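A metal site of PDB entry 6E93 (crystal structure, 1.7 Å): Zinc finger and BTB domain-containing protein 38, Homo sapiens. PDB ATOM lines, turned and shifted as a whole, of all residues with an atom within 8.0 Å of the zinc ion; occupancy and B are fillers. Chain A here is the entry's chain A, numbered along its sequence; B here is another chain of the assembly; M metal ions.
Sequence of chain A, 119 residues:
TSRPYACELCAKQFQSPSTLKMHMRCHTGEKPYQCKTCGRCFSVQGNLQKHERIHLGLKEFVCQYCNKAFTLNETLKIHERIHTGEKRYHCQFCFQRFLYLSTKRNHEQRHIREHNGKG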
ATOM      1  N   GLN A  34     -18.921 -17.590 -29.122  1.00  0.00           N
ATOM      2  CA  GLN A  34     -20.331 -17.952 -29.093  1.00  0.00           C
ATOM      3  C   GLN A  34     -20.644 -19.151 -29.974  1.00  0.00           C
ATOM      4  O   GLN A  34     -20.233 -19.222 -31.139  1.00  0.00           O
ATOM      5  CB  GLN A  34     -21.192 -16.761 -29.512  1.00  0.00           C
ATOM      6  CG  GLN A  34     -22.689 -17.085 -29.549  1.00  0.00           C
ATOM      7  CD  GLN A  34     -23.527 -15.858 -29.818  1.00  0.00           C
ATOM      8  OE1 GLN A  34     -23.308 -15.154 -30.790  1.00  0.00           O
ATOM      9  NE2 GLN A  34     -24.504 -15.598 -28.942  1.00  0.00           N
ATOM     10  N   CYS A  35     -21.393 -20.112 -29.418  1.00  0.00           N
ATOM     11  CA  CYS A  35     -21.801 -21.268 -30.183  1.00  0.00           C
ATOM     12  C   CYS A  35     -22.809 -20.839 -31.234  1.00  0.00           C
ATOM     13  O   CYS A  35     -23.808 -20.183 -30.918  1.00  0.00           O
ATOM     14  CB  CYS A  35     -22.419 -22.324 -29.268  1.00  0.00           C
ATOM     15  SG  CYS A  35     -23.168 -23.693 -30.181  1.00  0.00           S
ATOM     16  N   LYS A  36     -22.545 -21.190 -32.494  1.00  0.00           N
ATOM     17  CA  LYS A  36     -23.418 -20.732 -33.564  1.00  0.00           C
ATOM     18  C   LYS A  36     -24.742 -21.469 -33.592  1.00  0.00           C
ATOM     19  O   LYS A  36     -25.648 -21.046 -34.307  1.00  0.00           O
ATOM     20  CB  LYS A  36     -22.722 -20.882 -34.912  1.00  0.00           C
ATOM     21  CG  LYS A  36     -21.478 -20.002 -35.075  1.00  0.00           C
ATOM     22  CD  LYS A  36     -20.704 -20.403 -36.335  1.00  0.00           C
ATOM     23  CE  LYS A  36     -19.331 -19.747 -36.382  1.00  0.00           C
ATOM     24  NZ  LYS A  36     -19.426 -18.279 -36.527  1.00  0.00           N
ATOM     25  N   THR A  37     -24.879 -22.567 -32.846  1.00  0.00           N
ATOM     26  CA  THR A  37     -26.147 -23.283 -32.840  1.00  0.00           C
ATOM     27  C   THR A  37     -27.078 -22.758 -31.750  1.00  0.00           C
ATOM     28  O   THR A  37     -28.220 -22.364 -32.025  1.00  0.00           O
ATOM     29  CB  THR A  37     -25.924 -24.797 -32.678  1.00  0.00           C
ATOM     30  OG1 THR A  37     -25.185 -25.293 -33.809  1.00  0.00           O
ATOM     31  CG2 THR A  37     -27.247 -25.528 -32.582  1.00  0.00           C
ATOM     32  N   CYS A  38     -26.605 -22.762 -30.495  1.00  0.00           N
ATOM     33  CA  CYS A  38     -27.495 -22.454 -29.382  1.00  0.00           C
ATOM     34  C   CYS A  38     -27.237 -21.094 -28.769  1.00  0.00           C
ATOM     35  O   CYS A  38     -28.060 -20.624 -27.971  1.00  0.00           O
ATOM     36  CB  CYS A  38     -27.397 -23.538 -28.307  1.00  0.00           C
ATOM     37  SG  CYS A  38     -25.882 -23.458 -27.320  1.00  0.00           S
ATOM     38  N   GLY A  39     -26.163 -20.409 -29.159  1.00  0.00           N
ATOM     39  CA  GLY A  39     -25.924 -19.079 -28.659  1.00  0.00           C
ATOM     40  C   GLY A  39     -25.181 -19.002 -27.350  1.00  0.00           C
ATOM     41  O   GLY A  39     -24.839 -17.893 -26.924  1.00  0.00           O
ATOM     42  N   ARG A  40     -24.887 -20.139 -26.702  1.00  0.00           N
ATOM     43  CA  ARG A  40     -24.120 -20.100 -25.454  1.00  0.00           C
ATOM     44  C   ARG A  40     -22.725 -19.540 -25.734  1.00  0.00           C
ATOM     45  O   ARG A  40     -22.095 -19.869 -26.734  1.00  0.00           O
ATOM     46  CB  ARG A  40     -24.000 -21.480 -24.823  1.00  0.00           C
ATOM     47  CG  ARG A  40     -23.290 -21.458 -23.485  1.00  0.00           C
ATOM     48  CD  ARG A  40     -23.390 -22.800 -22.773  1.00  0.00           C
ATOM     49  NE  ARG A  40     -22.703 -22.690 -21.497  1.00  0.00           N
ATOM     50  CZ  ARG A  40     -23.119 -23.274 -20.371  1.00  0.00           C
ATOM     51  NH1 ARG A  40     -24.218 -24.024 -20.376  1.00  0.00           N
ATOM     52  NH2 ARG A  40     -22.425 -23.095 -19.255  1.00  0.00           N
ATOM     53  N   CYS A  41     -22.246 -18.695 -24.832  1.00  0.00           N
ATOM     54  CA  CYS A  41     -20.949 -18.048 -24.985  1.00  0.00           C
ATOM     55  C   CYS A  41     -19.944 -18.620 -24.001  1.00  0.00           C
ATOM     56  O   CYS A  41     -20.309 -19.078 -22.921  1.00  0.00           O
ATOM     57  CB  CYS A  41     -21.080 -16.538 -24.782  1.00  0.00           C
ATOM     58  SG  CYS A  41     -22.051 -15.763 -26.110  1.00  0.00           S
ATOM     59  N   PHE A  42     -18.661 -18.554 -24.383  1.00  0.00           N
ATOM     60  CA  PHE A  42     -17.586 -19.150 -23.592  1.00  0.00           C
ATOM     61  C   PHE A  42     -16.429 -18.170 -23.454  1.00  0.00           C
ATOM     62  O   PHE A  42     -16.129 -17.404 -24.376  1.00  0.00           O
ATOM     63  CB  PHE A  42     -17.061 -20.446 -24.258  1.00  0.00           C
ATOM     64  CG  PHE A  42     -18.043 -21.574 -24.217  1.00  0.00           C
ATOM     65  CD1 PHE A  42     -19.102 -21.610 -25.128  1.00  0.00           C
ATOM     66  CD2 PHE A  42     -17.940 -22.577 -23.271  1.00  0.00           C
ATOM     67  CE1 PHE A  42     -20.029 -22.638 -25.077  1.00  0.00           C
ATOM     68  CE2 PHE A  42     -18.853 -23.614 -23.224  1.00  0.00           C
ATOM     69  CZ  PHE A  42     -19.906 -23.641 -24.117  1.00  0.00           C
ATOM     70  N   LEU A  48     -15.459 -23.783 -26.052  1.00  0.00           N
ATOM     71  CA  LEU A  48     -16.536 -23.752 -27.034  1.00  0.00           C
ATOM     72  C   LEU A  48     -16.431 -24.945 -27.973  1.00  0.00           C
ATOM     73  O   LEU A  48     -17.420 -25.617 -28.264  1.00  0.00           O
ATOM     74  CB  LEU A  48     -16.509 -22.436 -27.818  1.00  0.00           C
ATOM     75  CG  LEU A  48     -17.439 -22.377 -29.034  1.00  0.00           C
ATOM     76  CD1 LEU A  48     -18.902 -22.637 -28.633  1.00  0.00           C
ATOM     77  CD2 LEU A  48     -17.283 -21.035 -29.732  1.00  0.00           C
ATOM     78  N   HIS A  51     -17.826 -27.950 -26.538  1.00  0.00           N
ATOM     79  CA  HIS A  51     -19.272 -27.818 -26.503  1.00  0.00           C
ATOM     80  C   HIS A  51     -19.876 -28.094 -27.868  1.00  0.00           C
ATOM     81  O   HIS A  51     -20.926 -28.744 -27.993  1.00  0.00           O
ATOM     82  CB  HIS A  51     -19.640 -26.418 -26.007  1.00  0.00           C
ATOM     83  CG  HIS A  51     -21.069 -26.067 -26.217  1.00  0.00           C
ATOM     84  ND1 HIS A  51     -22.057 -26.423 -25.333  1.00  0.00           N
ATOM     85  CD2 HIS A  51     -21.687 -25.448 -27.258  1.00  0.00           C
ATOM     86  CE1 HIS A  51     -23.224 -26.015 -25.810  1.00  0.00           C
ATOM     87  NE2 HIS A  51     -23.025 -25.414 -26.964  1.00  0.00           N
ATOM     88  N   GLU A  52     -19.237 -27.597 -28.922  1.00  0.00           N
ATOM     89  CA  GLU A  52     -19.816 -27.750 -30.242  1.00  0.00           C
ATOM     90  C   GLU A  52     -19.942 -29.215 -30.645  1.00  0.00           C
ATOM     91  O   GLU A  52     -20.838 -29.571 -31.414  1.00  0.00           O
ATOM     92  CB  GLU A  52     -19.005 -26.965 -31.267  1.00  0.00           C
ATOM     93  CG  GLU A  52     -19.153 -25.477 -31.069  1.00  0.00           C
ATOM     94  CD  GLU A  52     -18.192 -24.656 -31.933  1.00  0.00           C
ATOM     95  OE1 GLU A  52     -17.076 -25.139 -32.245  1.00  0.00           O
ATOM     96  OE2 GLU A  52     -18.559 -23.528 -32.281  1.00  0.00           O
ATOM     97  N   ARG A  53     -19.075 -30.081 -30.103  1.00  0.00           N
ATOM     98  CA  ARG A  53     -19.188 -31.493 -30.433  1.00  0.00           C
ATOM     99  C   ARG A  53     -20.536 -32.059 -30.017  1.00  0.00           C
ATOM    100  O   ARG A  53     -21.012 -33.035 -30.608  1.00  0.00           O
ATOM    101  CB  ARG A  53     -18.060 -32.280 -29.761  1.00  0.00           C
ATOM    102  CG  ARG A  53     -16.696 -32.003 -30.339  1.00  0.00           C
ATOM    103  CD  ARG A  53     -15.652 -32.831 -29.608  1.00  0.00           C
ATOM    104  NE  ARG A  53     -14.311 -32.575 -30.133  1.00  0.00           N
ATOM    105  CZ  ARG A  53     -13.760 -33.264 -31.117  1.00  0.00           C
ATOM    106  NH1 ARG A  53     -14.419 -34.258 -31.700  1.00  0.00           N
ATOM    107  NH2 ARG A  53     -12.541 -32.962 -31.528  1.00  0.00           N
ATOM    108  N   ILE A  54     -21.169 -31.470 -29.000  1.00  0.00           N
ATOM    109  CA  ILE A  54     -22.461 -31.968 -28.555  1.00  0.00           C
ATOM    110  C   ILE A  54     -23.494 -31.839 -29.670  1.00  0.00           C
ATOM    111  O   ILE A  54     -24.292 -32.750 -29.902  1.00  0.00           O
ATOM    112  CB  ILE A  54     -22.920 -31.247 -27.289  1.00  0.00           C
ATOM    113  CG1 ILE A  54     -21.892 -31.418 -26.175  1.00  0.00           C
ATOM    114  CG2 ILE A  54     -24.298 -31.773 -26.872  1.00  0.00           C
ATOM    115  CD1 ILE A  54     -22.166 -30.576 -24.937  1.00  0.00           C
ATOM    116  N   HIS A  55     -23.495 -30.696 -30.358  1.00  0.00           N
ATOM    117  CA  HIS A  55     -24.466 -30.475 -31.411  1.00  0.00           C
ATOM    118  C   HIS A  55     -24.203 -31.370 -32.622  1.00  0.00           C
ATOM    119  O   HIS A  55     -25.149 -31.769 -33.316  1.00  0.00           O
ATOM    120  CB  HIS A  55     -24.454 -29.001 -31.839  1.00  0.00           C
ATOM    121  CG  HIS A  55     -24.826 -28.059 -30.748  1.00  0.00           C
ATOM    122  ND1 HIS A  55     -25.971 -28.194 -29.991  1.00  0.00           N
ATOM    123  CD2 HIS A  55     -24.209 -26.943 -30.278  1.00  0.00           C
ATOM    124  CE1 HIS A  55     -26.034 -27.219 -29.099  1.00  0.00           C
ATOM    125  NE2 HIS A  55     -24.989 -26.432 -29.262  1.00  0.00           N
ATOM    126  N1  5CM B   9     -17.674 -28.138 -17.963  1.00  0.00           N
ATOM    127  C2  5CM B   9     -16.835 -28.417 -16.891  1.00  0.00           C
ATOM    128  N3  5CM B   9     -15.890 -29.392 -16.988  1.00  0.00           N
ATOM    129  C4  5CM B   9     -15.745 -30.081 -18.123  1.00  0.00           C
ATOM    130  C5  5CM B   9     -16.591 -29.800 -19.255  1.00  0.00           C
ATOM    131  C5A 5CM B   9     -16.460 -30.551 -20.571  1.00  0.00           C
ATOM    132  C6  5CM B   9     -17.557 -28.812 -19.141  1.00  0.00           C
ATOM    133  O2  5CM B   9     -16.991 -27.755 -15.873  1.00  0.00           O
ATOM    134  N4  5CM B   9     -14.814 -31.026 -18.195  1.00  0.00           N
ATOM    135  C1' 5CM B   9     -18.702 -27.106 -17.763  1.00  0.00           C
ATOM    136  C2' 5CM B   9     -18.171 -25.692 -17.734  1.00  0.00           C
ATOM    137  C3' 5CM B   9     -18.712 -25.118 -19.048  1.00  0.00           C
ATOM    138  C4' 5CM B   9     -19.973 -25.937 -19.267  1.00  0.00           C
ATOM    139  O4' 5CM B   9     -19.653 -27.262 -18.812  1.00  0.00           O
ATOM    140  O3' 5CM B   9     -19.030 -23.744 -18.930  1.00  0.00           O
ATOM    141  C5' 5CM B   9     -20.378 -26.013 -20.699  1.00  0.00           C
ATOM    142  O5' 5CM B   9     -21.792 -26.211 -20.812  1.00  0.00           O
ATOM    143  P   5CM B   9     -22.283 -27.430 -21.727  1.00  0.00           P
ATOM    144  OP1 5CM B   9     -23.722 -27.324 -22.013  1.00  0.00           O
ATOM    145  OP2 5CM B   9     -21.397 -27.552 -22.891  1.00  0.00           O
HETATM  146 ZN    ZN M   1     -24.314 -24.739 -28.456  1.00  0.00          ZN
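The zinc ion is bound by a ring nitrogen (NE2) of His 55 (2.0 Å), a ring nitrogen (NE2) of His 51 (2.1 Å), the side-chain sulfur (SG) of Cys 35 (2.3 Å) and the side-chain sulfur (SG) of Cys 38 (2.3 Å).
The zinc ion has four donor atoms within binding distance.
Four residues have an atom within 4 Å of the zinc ion: Cys 35, Cys 38, His 51 and His 55.
The nearest printed residue that does not touch the zinc ion is Thr 37 (4.5 Å).
N of Cys 35 lies within hydrogen-bond range of O of Arg 40 (2.8 Å).
SG of Cys 35 lies close to N of Thr 37 (3.4 Å).
N of Arg 40 lies close to SG of Cys 38 (3.5 Å).
ND1 of His 51 sits at hydrogen-bond distance from OP2 of 5CM 9 of chain B (2.8 Å).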
